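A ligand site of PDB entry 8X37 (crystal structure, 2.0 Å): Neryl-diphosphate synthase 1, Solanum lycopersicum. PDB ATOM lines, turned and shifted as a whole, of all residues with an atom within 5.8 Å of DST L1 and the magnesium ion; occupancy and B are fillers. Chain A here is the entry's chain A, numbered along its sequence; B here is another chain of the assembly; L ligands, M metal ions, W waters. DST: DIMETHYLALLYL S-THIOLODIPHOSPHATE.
The guanidinium group (NH1) of Arg 96 is in salt-bridge range of an oxygen (O8) of DST L1, 3.0 Å away. The backbone NH (N) of Arg 49 sits at hydrogen-bond distance from an oxygen (O6) of DST L1, at 3.0 Å. NE of Arg 49 lies within salt-bridge range of O6 of DST L1, at 2.9 Å. A ring nitrogen (NE2) of His 260 of chain B is in hydrogen-bond range of an oxygen (O5) of DST L1 (3.0 Å). O8 of DST L1 sits at hydrogen-bond distance from NE2 of His 62. The backbone NH (N) of Arg 48 sits at hydrogen-bond distance from an oxygen (O2) of DST L1, 3.1 Å away. An oxygen (O5) of DST L1 lies within salt-bridge range of the guanidinium group (NH1) of Arg 48, at 3.9 Å. N of Asn 47 sits at hydrogen-bond distance from O2 of DST L1 (3.4 Å). The side-chain amide nitrogen (ND2) of Asn 47 sits close to a sulfur (S9) of DST L1. N of Gly 46 lies close to S9 of DST L1 (3.4 Å). An oxygen (O4) of DST L1 lies close to the guanidinium group (NH1) of Arg 256 of chain B (3.7 Å). O8 of DST L2 lies within salt-bridge range of NH2 of Arg 96 (3.5 Å). NH1 of Arg 256 of chain B lies within salt-bridge range of O4 of DST L2 (3.2 Å). ND2 of Asn 93 sits at hydrogen-bond distance from O8 of DST L2, 3.0 Å away. The guanidinium group (NH2) of Arg 208 lies within salt-bridge range of an oxygen (O4) of DST L2 (3.2 Å).
NH2 of Arg 49 is in salt-bridge range of OD2 of Asp 45 (3.6 Å). The side-chain carboxylate of Asp 45 lies within salt-bridge range of the guanidinium group of Arg 208 (3.1 Å). OE2 of Glu 100 is in salt-bridge range of NH1 of Arg 96. ND1 of His 260 of chain B lies within hydrogen-bond range of OE1 of Glu 100, at 3.0 Å. The backbone carbonyl oxygen of Met 44 sits at hydrogen-bond distance from the side-chain amide nitrogen of Asn 47 (3.1 Å).
A sulfur (S9) of DST L1 sits close to the backbone carbonyl oxygen (O) of Met 44 (3.8 Å). Ile 65 touches DST L1. O of Ala 88 touches C14 of DST L1, 2.9 Å away. Hydrophobic or aromatic side chains that line DST L1: His 62, Ile 65 and His 260 of chain B. Within 4 Å of DST L1: Met 44, Asp 45, Gly 46, Asn 47, Arg 48, Arg 49, His 62, Ile 65, Ala 88, Arg 96, Arg 256 of chain B and His 260 of chain B. The nearest printed residue that does not touch DST L1 is Glu 100 (4.1 Å).
Merely in contact with the magnesium ion: Arg 96 and Arg 256 of chain B. Within 4 Å of the magnesium ion: Asp 45, Arg 96 and Arg 256 of chain B. The nearest printed residue that does not touch the magnesium ion is Arg 49 (4.3 Å).
The magnesium ion is bound by the side-chain carboxylate (OD1) of Asp 45 (1.9 Å), water W2 (2.0 Å), an oxygen (O4) of DST L1 (2.0 Å), water W1 (2.0 Å), an oxygen (O7) of DST L2 (2.1 Å) and an oxygen (O7) of DST L1 (2.4 Å). The magnesium ion has six donor atoms within binding distance.
Water W1 lies within hydrogen-bond range of NH1 of Arg 256 of chain B (2.9 Å), O5 of DST L1 (3.2 Å) and NH2 of Arg 96 (3.4 Å). Water W2 lies within hydrogen-bond range of the side-chain carboxylate of Asp 45 and an oxygen (O4) of DST L2.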
ATOM      1  N   MET A  44     -15.421  16.439  -0.904  1.00  0.00           N
ATOM      2  CA  MET A  44     -14.869  16.196  -2.226  1.00  0.00           C
ATOM      3  C   MET A  44     -13.619  15.340  -2.112  1.00  0.00           C
ATOM      4  O   MET A  44     -12.538  15.811  -2.450  1.00  0.00           O
ATOM      5  CB  MET A  44     -14.470  17.513  -2.895  1.00  0.00           C
ATOM      6  CG  MET A  44     -15.605  18.510  -3.069  1.00  0.00           C
ATOM      7  SD  MET A  44     -14.869  20.078  -3.594  1.00  0.00           S
ATOM      8  CE  MET A  44     -16.365  20.779  -4.289  1.00  0.00           C
ATOM      9  N   ASP A  45     -13.810  14.073  -1.737  1.00  0.00           N
ATOM     10  CA  ASP A  45     -12.695  13.202  -1.373  1.00  0.00           C
ATOM     11  C   ASP A  45     -12.396  12.257  -2.532  1.00  0.00           C
ATOM     12  O   ASP A  45     -13.275  12.020  -3.354  1.00  0.00           O
ATOM     13  CB  ASP A  45     -13.051  12.440  -0.099  1.00  0.00           C
ATOM     14  CG  ASP A  45     -11.906  11.751   0.643  1.00  0.00           C
ATOM     15  OD1 ASP A  45     -10.748  12.184   0.458  1.00  0.00           O
ATOM     16  OD2 ASP A  45     -12.192  10.753   1.383  1.00  0.00           O
ATOM     17  N   GLY A  46     -11.155  11.770  -2.625  1.00  0.00           N
ATOM     18  CA  GLY A  46     -10.795  10.736  -3.573  1.00  0.00           C
ATOM     19  C   GLY A  46      -9.750  11.172  -4.611  1.00  0.00           C
ATOM     20  O   GLY A  46      -9.284  10.368  -5.404  1.00  0.00           O
ATOM     21  N   ASN A  47      -9.304  12.436  -4.559  1.00  0.00           N
ATOM     22  CA  ASN A  47      -8.566  13.060  -5.642  1.00  0.00           C
ATOM     23  C   ASN A  47      -7.200  12.416  -5.827  1.00  0.00           C
ATOM     24  O   ASN A  47      -6.748  12.243  -6.965  1.00  0.00           O
ATOM     25  CB  ASN A  47      -8.394  14.556  -5.419  1.00  0.00           C
ATOM     26  CG  ASN A  47      -9.743  15.229  -5.327  1.00  0.00           C
ATOM     27  OD1 ASN A  47     -10.581  15.011  -6.202  1.00  0.00           O
ATOM     28  ND2 ASN A  47     -10.010  15.963  -4.252  1.00  0.00           N
ATOM     29  N   ARG A  48      -6.544  12.087  -4.710  1.00  0.00           N
ATOM     30  CA  ARG A  48      -5.206  11.525  -4.789  1.00  0.00           C
ATOM     31  C   ARG A  48      -5.272  10.104  -5.354  1.00  0.00           C
ATOM     32  O   ARG A  48      -4.495   9.755  -6.240  1.00  0.00           O
ATOM     33  CB  ARG A  48      -4.476  11.630  -3.441  1.00  0.00           C
ATOM     34  CG  ARG A  48      -3.406  10.555  -3.369  1.00  0.00           C
ATOM     35  CD  ARG A  48      -2.452  10.647  -2.203  1.00  0.00           C
ATOM     36  NE  ARG A  48      -1.574   9.484  -2.210  1.00  0.00           N
ATOM     37  CZ  ARG A  48      -1.947   8.207  -2.033  1.00  0.00           C
ATOM     38  NH1 ARG A  48      -3.169   7.926  -1.593  1.00  0.00           N
ATOM     39  NH2 ARG A  48      -1.090   7.227  -2.253  1.00  0.00           N
ATOM     40  N   ARG A  49      -6.178   9.275  -4.819  1.00  0.00           N
ATOM     41  CA  ARG A  49      -6.264   7.884  -5.252  1.00  0.00           C
ATOM     42  C   ARG A  49      -6.574   7.851  -6.744  1.00  0.00           C
ATOM     43  O   ARG A  49      -6.004   7.044  -7.469  1.00  0.00           O
ATOM     44  CB  ARG A  49      -7.283   7.074  -4.431  1.00  0.00           C
ATOM     45  CG  ARG A  49      -6.721   6.533  -3.120  1.00  0.00           C
ATOM     46  CD  ARG A  49      -7.800   6.131  -2.088  1.00  0.00           C
ATOM     47  NE  ARG A  49      -8.547   7.262  -1.522  1.00  0.00           N
ATOM     48  CZ  ARG A  49      -9.844   7.279  -1.179  1.00  0.00           C
ATOM     49  NH1 ARG A  49     -10.578   6.179  -1.222  1.00  0.00           N
ATOM     50  NH2 ARG A  49     -10.422   8.401  -0.752  1.00  0.00           N
ATOM     51  N   TRP A  50      -7.468   8.748  -7.200  1.00  0.00           N
ATOM     52  CA  TRP A  50      -7.858   8.841  -8.601  1.00  0.00           C
ATOM     53  C   TRP A  50      -6.648   9.028  -9.515  1.00  0.00           C
ATOM     54  O   TRP A  50      -6.520   8.352 -10.537  1.00  0.00           O
ATOM     55  CB  TRP A  50      -8.861   9.978  -8.791  1.00  0.00           C
ATOM     56  CG  TRP A  50      -9.315  10.155 -10.204  1.00  0.00           C
ATOM     57  CD1 TRP A  50     -10.430   9.627 -10.792  1.00  0.00           C
ATOM     58  CD2 TRP A  50      -8.690  10.991 -11.212  1.00  0.00           C
ATOM     59  NE1 TRP A  50     -10.524  10.049 -12.088  1.00  0.00           N
ATOM     60  CE2 TRP A  50      -9.493  10.892 -12.368  1.00  0.00           C
ATOM     61  CE3 TRP A  50      -7.553  11.795 -11.236  1.00  0.00           C
ATOM     62  CZ2 TRP A  50      -9.163  11.570 -13.548  1.00  0.00           C
ATOM     63  CZ3 TRP A  50      -7.238  12.461 -12.402  1.00  0.00           C
ATOM     64  CH2 TRP A  50      -8.044  12.356 -13.538  1.00  0.00           C
ATOM     65  N   HIS A  62      -5.758  16.830  -7.883  1.00  0.00           N
ATOM     66  CA  HIS A  62      -6.194  18.069  -7.255  1.00  0.00           C
ATOM     67  C   HIS A  62      -6.659  19.078  -8.298  1.00  0.00           C
ATOM     68  O   HIS A  62      -7.522  19.903  -8.012  1.00  0.00           O
ATOM     69  CB  HIS A  62      -5.094  18.613  -6.341  1.00  0.00           C
ATOM     70  CG  HIS A  62      -4.825  17.734  -5.171  1.00  0.00           C
ATOM     71  ND1 HIS A  62      -3.550  17.433  -4.744  1.00  0.00           N
ATOM     72  CD2 HIS A  62      -5.662  17.069  -4.360  1.00  0.00           C
ATOM     73  CE1 HIS A  62      -3.622  16.630  -3.686  1.00  0.00           C
ATOM     74  NE2 HIS A  62      -4.894  16.394  -3.439  1.00  0.00           N
ATOM     75  N   ILE A  65     -10.500  19.732  -8.994  1.00  0.00           N
ATOM     76  CA  ILE A  65     -11.401  20.097  -7.908  1.00  0.00           C
ATOM     77  C   ILE A  65     -12.299  21.263  -8.331  1.00  0.00           C
ATOM     78  O   ILE A  65     -13.522  21.138  -8.327  1.00  0.00           O
ATOM     79  CB  ILE A  65     -10.622  20.379  -6.608  1.00  0.00           C
ATOM     80  CG1 ILE A  65      -9.948  19.109  -6.097  1.00  0.00           C
ATOM     81  CG2 ILE A  65     -11.534  20.998  -5.546  1.00  0.00           C
ATOM     82  CD1 ILE A  65      -8.985  19.342  -4.953  1.00  0.00           C
ATOM     83  N   PHE A  87     -16.467  21.040   0.928  1.00  0.00           N
ATOM     84  CA  PHE A  87     -15.280  20.951   1.753  1.00  0.00           C
ATOM     85  C   PHE A  87     -14.074  20.893   0.825  1.00  0.00           C
ATOM     86  O   PHE A  87     -13.838  19.879   0.162  1.00  0.00           O
ATOM     87  CB  PHE A  87     -15.422  19.769   2.712  1.00  0.00           C
ATOM     88  CG  PHE A  87     -14.648  19.822   4.039  1.00  0.00           C
ATOM     89  CD1 PHE A  87     -14.044  20.984   4.499  1.00  0.00           C
ATOM     90  CD2 PHE A  87     -14.630  18.712   4.890  1.00  0.00           C
ATOM     91  CE1 PHE A  87     -13.389  21.006   5.737  1.00  0.00           C
ATOM     92  CE2 PHE A  87     -13.991  18.752   6.125  1.00  0.00           C
ATOM     93  CZ  PHE A  87     -13.364  19.901   6.539  1.00  0.00           C
ATOM     94  N   ALA A  88     -13.293  21.989   0.809  1.00  0.00           N
ATOM     95  CA  ALA A  88     -12.117  22.099  -0.032  1.00  0.00           C
ATOM     96  C   ALA A  88     -10.824  21.879   0.719  1.00  0.00           C
ATOM     97  O   ALA A  88      -9.871  21.391   0.117  1.00  0.00           O
ATOM     98  CB  ALA A  88     -12.121  23.457  -0.696  1.00  0.00           C
ATOM     99  N   PHE A  89     -10.735  22.292   1.994  1.00  0.00           N
ATOM    100  CA  PHE A  89      -9.502  22.099   2.780  1.00  0.00           C
ATOM    101  C   PHE A  89      -9.805  22.158   4.297  1.00  0.00           C
ATOM    102  O   PHE A  89     -10.449  23.113   4.762  1.00  0.00           O
ATOM    103  CB  PHE A  89      -8.492  23.179   2.363  1.00  0.00           C
ATOM    104  CG  PHE A  89      -7.070  22.997   2.869  1.00  0.00           C
ATOM    105  CD1 PHE A  89      -6.677  23.523   4.099  1.00  0.00           C
ATOM    106  CD2 PHE A  89      -6.129  22.298   2.128  1.00  0.00           C
ATOM    107  CE1 PHE A  89      -5.374  23.349   4.578  1.00  0.00           C
ATOM    108  CE2 PHE A  89      -4.834  22.132   2.599  1.00  0.00           C
ATOM    109  CZ  PHE A  89      -4.458  22.668   3.819  1.00  0.00           C
ATOM    110  N   ASN A  93      -5.770  19.190   7.287  1.00  0.00           N
ATOM    111  CA  ASN A  93      -5.034  18.994   6.046  1.00  0.00           C
ATOM    112  C   ASN A  93      -3.640  19.636   6.102  1.00  0.00           C
ATOM    113  O   ASN A  93      -2.766  19.316   5.311  1.00  0.00           O
ATOM    114  CB  ASN A  93      -5.867  19.476   4.852  1.00  0.00           C
ATOM    115  CG  ASN A  93      -7.013  18.552   4.505  1.00  0.00           C
ATOM    116  OD1 ASN A  93      -8.029  19.015   3.955  1.00  0.00           O
ATOM    117  ND2 ASN A  93      -6.890  17.265   4.800  1.00  0.00           N
ATOM    118  N   ARG A  96      -0.410  17.394   5.899  1.00  0.00           N
ATOM    119  CA  ARG A  96       0.180  16.831   4.700  1.00  0.00           C
ATOM    120  C   ARG A  96       1.543  17.489   4.445  1.00  0.00           C
ATOM    121  O   ARG A  96       1.909  18.454   5.126  1.00  0.00           O
ATOM    122  CB  ARG A  96      -0.861  16.960   3.582  1.00  0.00           C
ATOM    123  CG  ARG A  96      -2.090  16.097   3.856  1.00  0.00           C
ATOM    124  CD  ARG A  96      -3.217  16.356   2.886  1.00  0.00           C
ATOM    125  NE  ARG A  96      -4.305  15.365   2.976  1.00  0.00           N
ATOM    126  CZ  ARG A  96      -5.283  15.217   2.095  1.00  0.00           C
ATOM    127  NH1 ARG A  96      -5.311  15.936   0.974  1.00  0.00           N
ATOM    128  NH2 ARG A  96      -6.242  14.328   2.300  1.00  0.00           N
ATOM    129  N   GLU A 100       2.749  19.285  -0.959  1.00  0.00           N
ATOM    130  CA  GLU A 100       1.341  19.096  -1.300  1.00  0.00           C
ATOM    131  C   GLU A 100       0.521  20.309  -0.847  1.00  0.00           C
ATOM    132  O   GLU A 100      -0.372  20.770  -1.569  1.00  0.00           O
ATOM    133  CB  GLU A 100       0.790  17.783  -0.726  1.00  0.00           C
ATOM    134  CG  GLU A 100      -0.670  17.524  -1.090  1.00  0.00           C
ATOM    135  CD  GLU A 100      -1.301  16.231  -0.576  1.00  0.00           C
ATOM    136  OE1 GLU A 100      -0.578  15.356  -0.026  1.00  0.00           O
ATOM    137  OE2 GLU A 100      -2.539  16.088  -0.730  1.00  0.00           O
ATOM    138  N   LEU A 104      -1.760  23.028  -3.213  1.00  0.00           N
ATOM    139  CA  LEU A 104      -3.196  23.173  -3.056  1.00  0.00           C
ATOM    140  C   LEU A 104      -3.550  24.639  -2.846  1.00  0.00           C
ATOM    141  O   LEU A 104      -4.502  25.130  -3.462  1.00  0.00           O
ATOM    142  CB  LEU A 104      -3.722  22.309  -1.894  1.00  0.00           C
ATOM    143  CG  LEU A 104      -3.965  20.824  -2.196  1.00  0.00           C
ATOM    144  CD1 LEU A 104      -4.013  20.017  -0.914  1.00  0.00           C
ATOM    145  CD2 LEU A 104      -5.242  20.630  -2.957  1.00  0.00           C
ATOM    146  N   PHE A 108      -5.842  27.091  -5.290  1.00  0.00           N
ATOM    147  CA  PHE A 108      -7.127  27.676  -4.929  1.00  0.00           C
ATOM    148  C   PHE A 108      -7.268  29.110  -5.442  1.00  0.00           C
ATOM    149  O   PHE A 108      -8.367  29.661  -5.415  1.00  0.00           O
ATOM    150  CB  PHE A 108      -7.323  27.598  -3.407  1.00  0.00           C
ATOM    151  CG  PHE A 108      -7.649  26.204  -2.868  1.00  0.00           C
ATOM    152  CD1 PHE A 108      -8.308  25.257  -3.646  1.00  0.00           C
ATOM    153  CD2 PHE A 108      -7.317  25.852  -1.565  1.00  0.00           C
ATOM    154  CE1 PHE A 108      -8.592  23.997  -3.154  1.00  0.00           C
ATOM    155  CE2 PHE A 108      -7.612  24.594  -1.074  1.00  0.00           C
ATOM    156  CZ  PHE A 108      -8.232  23.674  -1.870  1.00  0.00           C
ATOM    157  N   ARG A 208     -20.785  12.302   0.192  1.00  0.00           N
ATOM    158  CA  ARG A 208     -19.340  12.166   0.321  1.00  0.00           C
ATOM    159  C   ARG A 208     -18.845  11.145  -0.713  1.00  0.00           C
ATOM    160  O   ARG A 208     -19.168   9.956  -0.649  1.00  0.00           O
ATOM    161  CB  ARG A 208     -18.906  11.784   1.751  1.00  0.00           C
ATOM    162  CG  ARG A 208     -17.402  11.513   1.858  1.00  0.00           C
ATOM    163  CD  ARG A 208     -16.854  11.273   3.242  1.00  0.00           C
ATOM    164  NE  ARG A 208     -15.385  11.186   3.242  1.00  0.00           N
ATOM    165  CZ  ARG A 208     -14.580  11.616   4.216  1.00  0.00           C
ATOM    166  NH1 ARG A 208     -15.050  12.286   5.259  1.00  0.00           N
ATOM    167  NH2 ARG A 208     -13.290  11.366   4.171  1.00  0.00           N
ATOM    168  N   ARG B 256      -7.267   8.116   8.084  1.00  0.00           N
ATOM    169  CA  ARG B 256      -6.118   8.965   7.773  1.00  0.00           C
ATOM    170  C   ARG B 256      -6.134  10.232   8.616  1.00  0.00           C
ATOM    171  O   ARG B 256      -5.113  10.917   8.686  1.00  0.00           O
ATOM    172  CB  ARG B 256      -6.014   9.342   6.288  1.00  0.00           C
ATOM    173  CG  ARG B 256      -5.790   8.120   5.408  1.00  0.00           C
ATOM    174  CD  ARG B 256      -5.923   8.427   3.915  1.00  0.00           C
ATOM    175  NE  ARG B 256      -6.694   7.382   3.238  1.00  0.00           N
ATOM    176  CZ  ARG B 256      -7.956   7.509   2.851  1.00  0.00           C
ATOM    177  NH1 ARG B 256      -8.608   8.648   2.985  1.00  0.00           N
ATOM    178  NH2 ARG B 256      -8.563   6.488   2.297  1.00  0.00           N
ATOM    179  N   HIS B 260      -1.876  11.659   5.131  1.00  0.00           N
ATOM    180  CA  HIS B 260      -1.612  10.807   3.977  1.00  0.00           C
ATOM    181  C   HIS B 260      -0.641   9.685   4.376  1.00  0.00           C
ATOM    182  O   HIS B 260       0.583   9.940   4.394  1.00  0.00           O
ATOM    183  CB  HIS B 260      -1.099  11.629   2.773  1.00  0.00           C
ATOM    184  CG  HIS B 260      -2.099  11.937   1.678  1.00  0.00           C
ATOM    185  ND1 HIS B 260      -1.735  12.587   0.511  1.00  0.00           N
ATOM    186  CD2 HIS B 260      -3.435  11.729   1.560  1.00  0.00           C
ATOM    187  CE1 HIS B 260      -2.809  12.764  -0.257  1.00  0.00           C
ATOM    188  NE2 HIS B 260      -3.843  12.229   0.354  1.00  0.00           N
HETATM  189  O4  DST L   1      -8.421  10.735  -0.117  1.00  0.00           O
HETATM  190  P1  DST L   1      -7.365  10.723  -1.171  1.00  0.00           P
HETATM  191  O6  DST L   1      -7.766   9.911  -2.356  1.00  0.00           O
HETATM  192  O5  DST L   1      -6.005  10.395  -0.634  1.00  0.00           O
HETATM  193  O2  DST L   1      -7.337  12.201  -1.747  1.00  0.00           O
HETATM  194  P3  DST L   1      -7.393  13.615  -1.031  1.00  0.00           P
HETATM  195  O8  DST L   1      -6.222  14.432  -1.487  1.00  0.00           O
HETATM  196  O7  DST L   1      -7.645  13.425   0.442  1.00  0.00           O
HETATM  197  S9  DST L   1      -9.166  14.358  -1.658  1.00  0.00           S
HETATM  198  C10 DST L   1      -9.599  15.367  -0.218  1.00  0.00           C
HETATM  199  C11 DST L   1     -10.133  16.664  -0.652  1.00  0.00           C
HETATM  200  C12 DST L   1      -9.441  17.762  -0.869  1.00  0.00           C
HETATM  201  C13 DST L   1      -7.979  17.905  -0.527  1.00  0.00           C
HETATM  202  C14 DST L   1     -10.060  18.959  -1.527  1.00  0.00           C
HETATM  203  O4  DST L   2     -10.377  10.484   4.986  1.00  0.00           O
HETATM  204  P1  DST L   2      -9.932  11.567   5.961  1.00  0.00           P
HETATM  205  O6  DST L   2      -8.457  11.510   6.224  1.00  0.00           O
HETATM  206  O5  DST L   2     -10.743  11.563   7.263  1.00  0.00           O
HETATM  207  O2  DST L   2     -10.265  12.990   5.328  1.00  0.00           O
HETATM  208  P3  DST L   2      -9.651  13.864   4.132  1.00  0.00           P
HETATM  209  O8  DST L   2      -8.758  14.923   4.665  1.00  0.00           O
HETATM  210  O7  DST L   2      -9.078  12.875   3.177  1.00  0.00           O
HETATM  211  S9  DST L   2     -11.446  14.649   3.578  1.00  0.00           S
HETATM  212  C10 DST L   2     -11.867  16.175   4.441  1.00  0.00           C
HETATM  213  C11 DST L   2     -11.376  17.343   3.705  1.00  0.00           C
HETATM  214  C12 DST L   2     -11.775  17.727   2.507  1.00  0.00           C
HETATM  215  C13 DST L   2     -11.261  18.973   1.876  1.00  0.00           C
HETATM  216  C14 DST L   2     -12.788  16.989   1.678  1.00  0.00           C
HETATM  217 MG    MG M   1      -9.114  11.834   1.410  1.00  0.00          MG
HETATM  218  O   HOH W   1      -7.388  11.135   2.158  1.00  0.00           O
HETATM  219  O   HOH W   2      -9.990  10.339   2.372  1.00  0.00           O
